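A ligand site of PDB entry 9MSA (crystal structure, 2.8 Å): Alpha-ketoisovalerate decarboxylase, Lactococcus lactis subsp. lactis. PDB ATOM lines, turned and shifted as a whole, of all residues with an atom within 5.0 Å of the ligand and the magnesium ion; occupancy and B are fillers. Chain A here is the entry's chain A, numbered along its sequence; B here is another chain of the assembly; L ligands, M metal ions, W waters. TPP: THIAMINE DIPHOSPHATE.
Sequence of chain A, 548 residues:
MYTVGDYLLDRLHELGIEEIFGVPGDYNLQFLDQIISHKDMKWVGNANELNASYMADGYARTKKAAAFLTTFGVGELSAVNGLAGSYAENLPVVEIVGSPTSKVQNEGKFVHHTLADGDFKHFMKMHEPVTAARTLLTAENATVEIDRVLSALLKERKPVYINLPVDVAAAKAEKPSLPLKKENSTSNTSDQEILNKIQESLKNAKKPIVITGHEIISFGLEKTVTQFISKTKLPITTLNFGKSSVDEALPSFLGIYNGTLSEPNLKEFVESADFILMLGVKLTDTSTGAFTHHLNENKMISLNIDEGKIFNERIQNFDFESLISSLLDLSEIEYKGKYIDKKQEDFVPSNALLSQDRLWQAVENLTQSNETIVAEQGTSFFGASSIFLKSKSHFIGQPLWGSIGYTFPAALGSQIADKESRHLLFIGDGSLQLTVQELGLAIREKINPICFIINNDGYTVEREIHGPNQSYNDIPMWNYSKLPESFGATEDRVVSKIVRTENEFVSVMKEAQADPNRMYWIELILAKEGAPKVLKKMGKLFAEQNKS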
ATOM      1  N   TYR A  54     -40.711 -23.870 -23.095  1.00  0.00           N
ATOM      2  CA  TYR A  54     -39.559 -24.002 -23.973  1.00  0.00           C
ATOM      3  C   TYR A  54     -40.025 -24.509 -25.336  1.00  0.00           C
ATOM      4  O   TYR A  54     -39.515 -24.074 -26.364  1.00  0.00           O
ATOM      5  CB  TYR A  54     -38.621 -25.055 -23.415  1.00  0.00           C
ATOM      6  CG  TYR A  54     -37.752 -24.708 -22.210  1.00  0.00           C
ATOM      7  CD1 TYR A  54     -37.519 -23.392 -21.800  1.00  0.00           C
ATOM      8  CD2 TYR A  54     -37.111 -25.713 -21.506  1.00  0.00           C
ATOM      9  CE1 TYR A  54     -36.676 -23.102 -20.746  1.00  0.00           C
ATOM     10  CE2 TYR A  54     -36.267 -25.436 -20.441  1.00  0.00           C
ATOM     11  CZ  TYR A  54     -36.060 -24.128 -20.038  1.00  0.00           C
ATOM     12  OH  TYR A  54     -35.237 -23.932 -18.978  1.00  0.00           O
ATOM     13  N   GLN A 377     -26.360 -24.555 -25.268  1.00  0.00           N
ATOM     14  CA  GLN A 377     -25.200 -23.880 -24.692  1.00  0.00           C
ATOM     15  C   GLN A 377     -24.235 -24.943 -24.169  1.00  0.00           C
ATOM     16  O   GLN A 377     -24.664 -25.959 -23.641  1.00  0.00           O
ATOM     17  CB  GLN A 377     -25.571 -22.892 -23.592  1.00  0.00           C
ATOM     18  CG  GLN A 377     -26.419 -21.718 -24.054  1.00  0.00           C
ATOM     19  CD  GLN A 377     -25.822 -20.915 -25.197  1.00  0.00           C
ATOM     20  OE1 GLN A 377     -24.823 -20.212 -25.049  1.00  0.00           O
ATOM     21  NE2 GLN A 377     -26.478 -21.007 -26.348  1.00  0.00           N
ATOM     22  N   GLY A 378     -22.932 -24.682 -24.316  1.00  0.00           N
ATOM     23  CA  GLY A 378     -21.887 -25.654 -24.021  1.00  0.00           C
ATOM     24  C   GLY A 378     -21.187 -25.979 -25.330  1.00  0.00           C
ATOM     25  O   GLY A 378     -21.383 -25.266 -26.314  1.00  0.00           O
ATOM     26  N   THR A 379     -20.391 -27.054 -25.329  1.00  0.00           N
ATOM     27  CA  THR A 379     -19.560 -27.424 -26.477  1.00  0.00           C
ATOM     28  C   THR A 379     -20.388 -27.384 -27.759  1.00  0.00           C
ATOM     29  O   THR A 379     -19.910 -26.899 -28.786  1.00  0.00           O
ATOM     30  CB  THR A 379     -18.883 -28.772 -26.267  1.00  0.00           C
ATOM     31  OG1 THR A 379     -19.867 -29.793 -26.138  1.00  0.00           O
ATOM     32  CG2 THR A 379     -17.963 -28.794 -25.064  1.00  0.00           C
ATOM     33  N   SER A 380     -21.635 -27.849 -27.677  1.00  0.00           N
ATOM     34  CA  SER A 380     -22.531 -27.984 -28.820  1.00  0.00           C
ATOM     35  C   SER A 380     -22.758 -26.651 -29.530  1.00  0.00           C
ATOM     36  O   SER A 380     -22.571 -26.557 -30.734  1.00  0.00           O
ATOM     37  CB  SER A 380     -23.835 -28.639 -28.451  1.00  0.00           C
ATOM     38  OG  SER A 380     -23.639 -29.778 -27.617  1.00  0.00           O
ATOM     39  N   GLY A 402     -29.791 -18.269 -22.492  1.00  0.00           N
ATOM     40  CA  GLY A 402     -28.742 -19.214 -22.155  1.00  0.00           C
ATOM     41  C   GLY A 402     -29.205 -20.202 -21.108  1.00  0.00           C
ATOM     42  O   GLY A 402     -28.424 -20.563 -20.228  1.00  0.00           O
ATOM     43  N   SER A 403     -30.464 -20.626 -21.195  1.00  0.00           N
ATOM     44  CA  SER A 403     -31.040 -21.541 -20.232  1.00  0.00           C
ATOM     45  C   SER A 403     -30.800 -22.975 -20.709  1.00  0.00           C
ATOM     46  O   SER A 403     -31.358 -23.374 -21.736  1.00  0.00           O
ATOM     47  CB  SER A 403     -32.501 -21.228 -20.082  1.00  0.00           C
ATOM     48  OG  SER A 403     -33.156 -22.216 -19.284  1.00  0.00           O
ATOM     49  N   ILE A 404     -29.997 -23.762 -19.974  1.00  0.00           N
ATOM     50  CA  ILE A 404     -29.689 -25.109 -20.434  1.00  0.00           C
ATOM     51  C   ILE A 404     -30.893 -26.032 -20.251  1.00  0.00           C
ATOM     52  O   ILE A 404     -31.652 -25.938 -19.288  1.00  0.00           O
ATOM     53  CB  ILE A 404     -28.416 -25.679 -19.791  1.00  0.00           C
ATOM     54  CG1 ILE A 404     -28.524 -25.829 -18.306  1.00  0.00           C
ATOM     55  CG2 ILE A 404     -27.174 -24.887 -20.169  1.00  0.00           C
ATOM     56  CD1 ILE A 404     -27.372 -26.631 -17.746  1.00  0.00           C
ATOM     57  N   GLY A 428     -25.921 -31.384 -24.828  1.00  0.00           N
ATOM     58  CA  GLY A 428     -24.952 -32.017 -23.946  1.00  0.00           C
ATOM     59  C   GLY A 428     -25.676 -32.855 -22.889  1.00  0.00           C
ATOM     60  O   GLY A 428     -26.850 -32.624 -22.578  1.00  0.00           O
ATOM     61  N   ASP A 429     -24.946 -33.841 -22.337  1.00  0.00           N
ATOM     62  CA  ASP A 429     -25.431 -34.716 -21.277  1.00  0.00           C
ATOM     63  C   ASP A 429     -25.980 -33.882 -20.109  1.00  0.00           C
ATOM     64  O   ASP A 429     -27.091 -34.119 -19.620  1.00  0.00           O
ATOM     65  CB  ASP A 429     -24.349 -35.707 -20.899  1.00  0.00           C
ATOM     66  CG  ASP A 429     -23.012 -35.147 -20.429  1.00  0.00           C
ATOM     67  OD1 ASP A 429     -22.725 -33.968 -20.749  1.00  0.00           O
ATOM     68  OD2 ASP A 429     -22.285 -35.891 -19.716  1.00  0.00           O
ATOM     69  N   GLY A 430     -25.213 -32.874 -19.696  1.00  0.00           N
ATOM     70  CA  GLY A 430     -25.585 -31.998 -18.606  1.00  0.00           C
ATOM     71  C   GLY A 430     -26.957 -31.398 -18.829  1.00  0.00           C
ATOM     72  O   GLY A 430     -27.785 -31.417 -17.935  1.00  0.00           O
ATOM     73  N   SER A 431     -27.199 -30.870 -20.031  1.00  0.00           N
ATOM     74  CA  SER A 431     -28.415 -30.146 -20.348  1.00  0.00           C
ATOM     75  C   SER A 431     -29.612 -31.074 -20.496  1.00  0.00           C
ATOM     76  O   SER A 431     -30.701 -30.730 -20.091  1.00  0.00           O
ATOM     77  CB  SER A 431     -28.254 -29.326 -21.589  1.00  0.00           C
ATOM     78  OG  SER A 431     -27.273 -28.331 -21.418  1.00  0.00           O
ATOM     79  N   LEU A 434     -32.117 -31.745 -17.758  1.00  0.00           N
ATOM     80  CA  LEU A 434     -33.081 -30.770 -17.275  1.00  0.00           C
ATOM     81  C   LEU A 434     -34.470 -31.060 -17.855  1.00  0.00           C
ATOM     82  O   LEU A 434     -35.465 -30.764 -17.206  1.00  0.00           O
ATOM     83  CB  LEU A 434     -32.677 -29.314 -17.494  1.00  0.00           C
ATOM     84  CG  LEU A 434     -31.589 -28.774 -16.553  1.00  0.00           C
ATOM     85  CD1 LEU A 434     -30.203 -29.054 -17.085  1.00  0.00           C
ATOM     86  CD2 LEU A 434     -31.760 -27.281 -16.285  1.00  0.00           C
ATOM     87  N   ILE A 454     -24.289 -35.215 -26.495  1.00  0.00           N
ATOM     88  CA  ILE A 454     -22.841 -35.179 -26.392  1.00  0.00           C
ATOM     89  C   ILE A 454     -22.436 -35.516 -24.963  1.00  0.00           C
ATOM     90  O   ILE A 454     -22.481 -34.663 -24.073  1.00  0.00           O
ATOM     91  CB  ILE A 454     -22.295 -33.841 -26.893  1.00  0.00           C
ATOM     92  CG1 ILE A 454     -22.707 -33.625 -28.333  1.00  0.00           C
ATOM     93  CG2 ILE A 454     -20.770 -33.777 -26.708  1.00  0.00           C
ATOM     94  CD1 ILE A 454     -22.369 -32.261 -28.880  1.00  0.00           C
ATOM     95  N   ASN A 456     -19.875 -36.157 -22.499  1.00  0.00           N
ATOM     96  CA  ASN A 456     -18.516 -35.777 -22.135  1.00  0.00           C
ATOM     97  C   ASN A 456     -18.426 -35.752 -20.619  1.00  0.00           C
ATOM     98  O   ASN A 456     -17.614 -35.018 -20.035  1.00  0.00           O
ATOM     99  CB  ASN A 456     -18.106 -34.469 -22.807  1.00  0.00           C
ATOM    100  CG  ASN A 456     -19.028 -33.304 -22.553  1.00  0.00           C
ATOM    101  OD1 ASN A 456     -19.915 -33.357 -21.684  1.00  0.00           O
ATOM    102  ND2 ASN A 456     -18.838 -32.234 -23.301  1.00  0.00           N
ATOM    103  N   GLY A 458     -20.202 -34.746 -17.963  1.00  0.00           N
ATOM    104  CA  GLY A 458     -20.337 -33.549 -17.154  1.00  0.00           C
ATOM    105  C   GLY A 458     -20.516 -32.263 -17.964  1.00  0.00           C
ATOM    106  O   GLY A 458     -20.828 -32.292 -19.157  1.00  0.00           O
ATOM    107  N   TYR A 459     -20.366 -31.149 -17.242  1.00  0.00           N
ATOM    108  CA  TYR A 459     -20.470 -29.794 -17.753  1.00  0.00           C
ATOM    109  C   TYR A 459     -19.077 -29.327 -18.189  1.00  0.00           C
ATOM    110  O   TYR A 459     -18.340 -28.742 -17.385  1.00  0.00           O
ATOM    111  CB  TYR A 459     -20.892 -28.966 -16.541  1.00  0.00           C
ATOM    112  CG  TYR A 459     -22.221 -29.238 -15.852  1.00  0.00           C
ATOM    113  CD1 TYR A 459     -23.331 -29.647 -16.572  1.00  0.00           C
ATOM    114  CD2 TYR A 459     -22.378 -29.029 -14.477  1.00  0.00           C
ATOM    115  CE1 TYR A 459     -24.557 -29.852 -15.949  1.00  0.00           C
ATOM    116  CE2 TYR A 459     -23.594 -29.217 -13.851  1.00  0.00           C
ATOM    117  CZ  TYR A 459     -24.686 -29.644 -14.588  1.00  0.00           C
ATOM    118  OH  TYR A 459     -25.900 -29.872 -14.012  1.00  0.00           O
ATOM    119  N   THR A 460     -18.711 -29.594 -19.455  1.00  0.00           N
ATOM    120  CA  THR A 460     -17.384 -29.276 -19.959  1.00  0.00           C
ATOM    121  C   THR A 460     -17.185 -27.767 -20.006  1.00  0.00           C
ATOM    122  O   THR A 460     -16.143 -27.275 -19.553  1.00  0.00           O
ATOM    123  CB  THR A 460     -17.130 -29.964 -21.301  1.00  0.00           C
ATOM    124  OG1 THR A 460     -16.743 -31.272 -20.901  1.00  0.00           O
ATOM    125  CG2 THR A 460     -15.952 -29.372 -22.067  1.00  0.00           C
ATOM    126  N   VAL A 461     -18.176 -27.034 -20.522  1.00  0.00           N
ATOM    127  CA  VAL A 461     -18.059 -25.584 -20.653  1.00  0.00           C
ATOM    128  C   VAL A 461     -17.739 -24.964 -19.299  1.00  0.00           C
ATOM    129  O   VAL A 461     -16.904 -24.062 -19.218  1.00  0.00           O
ATOM    130  CB  VAL A 461     -19.263 -24.910 -21.329  1.00  0.00           C
ATOM    131  CG1 VAL A 461     -20.534 -24.997 -20.471  1.00  0.00           C
ATOM    132  CG2 VAL A 461     -18.993 -23.458 -21.667  1.00  0.00           C
ATOM    133  N   GLU A 462     -18.414 -25.442 -18.233  1.00  0.00           N
ATOM    134  CA  GLU A 462     -18.162 -24.980 -16.875  1.00  0.00           C
ATOM    135  C   GLU A 462     -16.728 -25.306 -16.482  1.00  0.00           C
ATOM    136  O   GLU A 462     -16.053 -24.464 -15.905  1.00  0.00           O
ATOM    137  CB  GLU A 462     -19.095 -25.582 -15.815  1.00  0.00           C
ATOM    138  CG  GLU A 462     -20.581 -25.330 -16.045  1.00  0.00           C
ATOM    139  CD  GLU A 462     -20.998 -23.877 -16.123  1.00  0.00           C
ATOM    140  OE1 GLU A 462     -21.793 -23.535 -15.245  1.00  0.00           O
ATOM    141  OE2 GLU A 462     -20.557 -23.103 -17.018  1.00  0.00           O
ATOM    142  N   VAL B  23     -27.804 -25.936  -8.680  1.00  0.00           N
ATOM    143  CA  VAL B  23     -27.244 -26.219  -9.997  1.00  0.00           C
ATOM    144  C   VAL B  23     -26.178 -25.161 -10.301  1.00  0.00           C
ATOM    145  O   VAL B  23     -26.455 -23.964 -10.214  1.00  0.00           O
ATOM    146  CB  VAL B  23     -28.316 -26.231 -11.106  1.00  0.00           C
ATOM    147  CG1 VAL B  23     -27.718 -26.400 -12.496  1.00  0.00           C
ATOM    148  CG2 VAL B  23     -29.435 -27.234 -10.837  1.00  0.00           C
ATOM    149  N   PRO B  24     -24.953 -25.569 -10.689  1.00  0.00           N
ATOM    150  CA  PRO B  24     -23.889 -24.614 -10.982  1.00  0.00           C
ATOM    151  C   PRO B  24     -24.207 -23.739 -12.177  1.00  0.00           C
ATOM    152  O   PRO B  24     -24.904 -24.159 -13.086  1.00  0.00           O
ATOM    153  CB  PRO B  24     -22.695 -25.463 -11.353  1.00  0.00           C
ATOM    154  CG  PRO B  24     -23.030 -26.819 -10.795  1.00  0.00           C
ATOM    155  CD  PRO B  24     -24.523 -26.965 -10.835  1.00  0.00           C
ATOM    156  N   GLY B  25     -23.679 -22.520 -12.132  1.00  0.00           N
ATOM    157  CA  GLY B  25     -23.607 -21.652 -13.293  1.00  0.00           C
ATOM    158  C   GLY B  25     -22.371 -20.774 -13.176  1.00  0.00           C
ATOM    159  O   GLY B  25     -21.762 -20.704 -12.110  1.00  0.00           O
ATOM    160  N   ASP B  26     -22.017 -20.101 -14.259  1.00  0.00           N
ATOM    161  CA  ASP B  26     -20.784 -19.331 -14.266  1.00  0.00           C
ATOM    162  C   ASP B  26     -20.774 -18.301 -13.125  1.00  0.00           C
ATOM    163  O   ASP B  26     -19.723 -18.082 -12.542  1.00  0.00           O
ATOM    164  CB  ASP B  26     -20.467 -18.804 -15.647  1.00  0.00           C
ATOM    165  CG  ASP B  26     -21.494 -17.841 -16.196  1.00  0.00           C
ATOM    166  OD1 ASP B  26     -22.712 -18.204 -16.222  1.00  0.00           O
ATOM    167  OD2 ASP B  26     -21.060 -16.731 -16.589  1.00  0.00           O
ATOM    168  N   GLU B  49     -33.024 -26.742 -11.485  1.00  0.00           N
ATOM    169  CA  GLU B  49     -33.214 -25.828 -10.377  1.00  0.00           C
ATOM    170  C   GLU B  49     -34.568 -26.042  -9.694  1.00  0.00           C
ATOM    171  O   GLU B  49     -34.633 -25.975  -8.470  1.00  0.00           O
ATOM    172  CB  GLU B  49     -33.069 -24.376 -10.821  1.00  0.00           C
ATOM    173  CG  GLU B  49     -31.632 -23.959 -11.131  1.00  0.00           C
ATOM    174  CD  GLU B  49     -31.095 -24.300 -12.525  1.00  0.00           C
ATOM    175  OE1 GLU B  49     -31.818 -24.899 -13.366  1.00  0.00           O
ATOM    176  OE2 GLU B  49     -29.939 -23.926 -12.765  1.00  0.00           O
ATOM    177  N   THR B  71     -28.206 -19.888 -10.344  1.00  0.00           N
ATOM    178  CA  THR B  71     -27.504 -18.852 -11.089  1.00  0.00           C
ATOM    179  C   THR B  71     -28.516 -17.769 -11.490  1.00  0.00           C
ATOM    180  O   THR B  71     -29.700 -18.062 -11.662  1.00  0.00           O
ATOM    181  CB  THR B  71     -26.789 -19.486 -12.276  1.00  0.00           C
ATOM    182  OG1 THR B  71     -25.946 -18.474 -12.805  1.00  0.00           O
ATOM    183  CG2 THR B  71     -27.747 -19.986 -13.348  1.00  0.00           C
ATOM    184  N   VAL B  74     -31.751 -17.537 -15.219  1.00  0.00           N
ATOM    185  CA  VAL B  74     -32.223 -18.848 -15.653  1.00  0.00           C
ATOM    186  C   VAL B  74     -32.415 -19.783 -14.450  1.00  0.00           C
ATOM    187  O   VAL B  74     -33.353 -20.564 -14.425  1.00  0.00           O
ATOM    188  CB  VAL B  74     -31.309 -19.481 -16.703  1.00  0.00           C
ATOM    189  CG1 VAL B  74     -31.282 -18.664 -17.980  1.00  0.00           C
ATOM    190  CG2 VAL B  74     -29.909 -19.738 -16.175  1.00  0.00           C
ATOM    191  N   GLY B  75     -31.509 -19.688 -13.470  1.00  0.00           N
ATOM    192  CA  GLY B  75     -31.583 -20.566 -12.319  1.00  0.00           C
ATOM    193  C   GLY B  75     -32.735 -20.178 -11.382  1.00  0.00           C
ATOM    194  O   GLY B  75     -33.570 -21.013 -11.028  1.00  0.00           O
ATOM    195  N   SER B  78     -36.218 -20.604 -12.674  1.00  0.00           N
ATOM    196  CA  SER B  78     -36.634 -21.989 -12.780  1.00  0.00           C
ATOM    197  C   SER B  78     -37.208 -22.465 -11.438  1.00  0.00           C
ATOM    198  O   SER B  78     -38.157 -23.264 -11.406  1.00  0.00           O
ATOM    199  CB  SER B  78     -35.503 -22.862 -13.230  1.00  0.00           C
ATOM    200  OG  SER B  78     -35.167 -22.600 -14.582  1.00  0.00           O
ATOM    201  N   HIS B 113     -28.116 -14.447 -19.493  1.00  0.00           N
ATOM    202  CA  HIS B 113     -29.084 -14.609 -18.428  1.00  0.00           C
ATOM    203  C   HIS B 113     -29.722 -13.267 -18.068  1.00  0.00           C
ATOM    204  O   HIS B 113     -30.170 -13.086 -16.938  1.00  0.00           O
ATOM    205  CB  HIS B 113     -28.495 -15.324 -17.202  1.00  0.00           C
ATOM    206  CG  HIS B 113     -27.815 -16.636 -17.438  1.00  0.00           C
ATOM    207  ND1 HIS B 113     -27.873 -17.365 -18.595  1.00  0.00           N
ATOM    208  CD2 HIS B 113     -27.013 -17.334 -16.600  1.00  0.00           C
ATOM    209  CE1 HIS B 113     -27.143 -18.468 -18.456  1.00  0.00           C
ATOM    210  NE2 HIS B 113     -26.605 -18.470 -17.243  1.00  0.00           N
HETATM  211  N1' TPP L   1     -28.998 -23.685 -15.445  1.00  0.00           N
HETATM  212  C2' TPP L   1     -29.581 -23.207 -16.542  1.00  0.00           C
HETATM  213  CM2 TPP L   1     -31.063 -23.358 -16.672  1.00  0.00           C
HETATM  214  N3' TPP L   1     -28.945 -22.602 -17.547  1.00  0.00           N
HETATM  215  C4' TPP L   1     -27.611 -22.441 -17.416  1.00  0.00           C
HETATM  216  N4' TPP L   1     -26.979 -21.791 -18.402  1.00  0.00           N
HETATM  217  C5' TPP L   1     -26.903 -22.911 -16.285  1.00  0.00           C
HETATM  218  C6' TPP L   1     -27.658 -23.537 -15.322  1.00  0.00           C
HETATM  219  C7' TPP L   1     -25.386 -22.783 -16.197  1.00  0.00           C
HETATM  220  N3  TPP L   1     -24.712 -23.537 -17.269  1.00  0.00           N
HETATM  221  C2  TPP L   1     -24.474 -23.051 -18.537  1.00  0.00           C
HETATM  222  S1  TPP L   1     -23.742 -24.192 -19.589  1.00  0.00           S
HETATM  223  C5  TPP L   1     -23.709 -25.364 -18.364  1.00  0.00           C
HETATM  224  C4  TPP L   1     -24.270 -24.870 -17.164  1.00  0.00           C
HETATM  225  CM4 TPP L   1     -24.404 -25.651 -15.896  1.00  0.00           C
HETATM  226  C6  TPP L   1     -23.103 -26.696 -18.587  1.00  0.00           C
HETATM  227  C7  TPP L   1     -23.625 -27.388 -19.788  1.00  0.00           C
HETATM  228  O7  TPP L   1     -23.059 -28.731 -19.763  1.00  0.00           O
HETATM  229  PA  TPP L   1     -23.403 -29.775 -20.921  1.00  0.00           P
HETATM  230  O1A TPP L   1     -22.879 -31.115 -20.484  1.00  0.00           O
HETATM  231  O2A TPP L   1     -24.821 -29.620 -21.380  1.00  0.00           O
HETATM  232  O3A TPP L   1     -22.435 -29.170 -22.055  1.00  0.00           O
HETATM  233  PB  TPP L   1     -20.949 -29.597 -22.486  1.00  0.00           P
HETATM  234  O1B TPP L   1     -20.174 -28.290 -22.551  1.00  0.00           O
HETATM  235  O2B TPP L   1     -21.235 -30.236 -23.830  1.00  0.00           O
HETATM  236  O3B TPP L   1     -20.431 -30.570 -21.443  1.00  0.00           O
HETATM  237 MG    MG M   1     -21.697 -32.328 -21.599  1.00  0.00          MG
HETATM  238  O   HOH W   1     -22.296 -21.024 -17.536  1.00  0.00           O
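A nitrogen (N4') of the ligand lies within hydrogen-bond range of the backbone carbonyl oxygen of Gly 402 (2.6 Å). The backbone NH (N) of Thr 379 sits at hydrogen-bond distance from an oxygen (O1B) of the ligand, at 3.0 Å. An oxygen (O2B) of the ligand sits at hydrogen-bond distance from the side-chain hydroxyl of Thr 379 (2.7 Å). The backbone NH of Ser 431 sits at hydrogen-bond distance from an oxygen (O2A) of the ligand, at 3.0 Å. The side-chain hydroxyl of Ser 431 lies within hydrogen-bond range of an oxygen (O2A) of the ligand (2.8 Å). The backbone NH of Thr 460 sits close to an oxygen (O3B) of the ligand, at 2.8 Å. A nitrogen (N1') of the ligand lies within hydrogen-bond range of the side-chain carboxylate of Glu 49 of chain B. A nitrogen (N3') of the ligand lies within hydrogen-bond range of the backbone NH (N) of Ile 404 (2.9 Å). O1A of the ligand lies close to N of Gly 430 (3.0 Å). An oxygen (O1B) of the ligand sits at hydrogen-bond distance from the backbone NH of Val 461 (3.1 Å).
The side-chain amide nitrogen (ND2) of Asn 456 sits at hydrogen-bond distance from the side-chain hydroxyl (OG1) of Thr 460 (3.3 Å). O of Ile 454 sits at hydrogen-bond distance from N of Asp 429. The side-chain hydroxyl (OG) of Ser 78 of chain B sits at hydrogen-bond distance from the backbone carbonyl oxygen (O) of Val 74 of chain B (2.7 Å). OG of Ser 403 lies within hydrogen-bond range of OH of Tyr 54, 2.7 Å away.
Residues that only touch the magnesium ion: Ile 454. Within 4 Å of the magnesium ion: Asp 429, Ile 454, Asn 456 and Gly 458.
An oxygen (O1A) of the ligand binds the magnesium ion, 2.0 Å away. The side-chain amide oxygen (OD1) of Asn 456 is bound to the magnesium ion (2.1 Å). The side-chain carboxylate (OD1) of Asp 429 is bound to the magnesium ion (2.1 Å). O3B of the ligand is bound to the magnesium ion (2.2 Å). The magnesium ion is bound by O of Gly 458 (2.6 Å). The magnesium ion has five donor atoms within binding distance.
Gly 378 touches the ligand. Ser 403 touches the ligand. Gly 428 touches the ligand (CA to O2A, 3.5 Å). Tyr 459 touches the ligand. OE1 of Glu 462 touches C4 of the ligand, 3.4 Å away. Pro 24 of chain B touches the ligand (O to CM4, 3.2 Å). Gly 25 of chain B touches the ligand (CA to C7', 3.6 Å). Val 74 of chain B touches the ligand (CG2 to N3', 3.3 Å). His 113 of chain B touches the ligand. Hydrophobic or aromatic side chains within 4 Å of the ligand: Ile 404, Tyr 459, Val 461, Val 74 of chain B and His 113 of chain B. 20 residues have an atom within 4 Å of the ligand: Gly 378, Thr 379, Gly 402, Ser 403, Ile 404, Gly 428, Asp 429, Gly 430, Ser 431, Asn 456, Gly 458, Tyr 459, Thr 460, Val 461, Glu 462, Pro 24 of chain B, Gly 25 of chain B, Glu 49 of chain B, Val 74 of chain B and His 113 of chain B.
Water W1 bridges the side-chain carboxylate (OE2) of Glu 462 (2.8 Å) and the side-chain carboxylate (OD1) of Asp 26 of chain B (3.1 Å).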
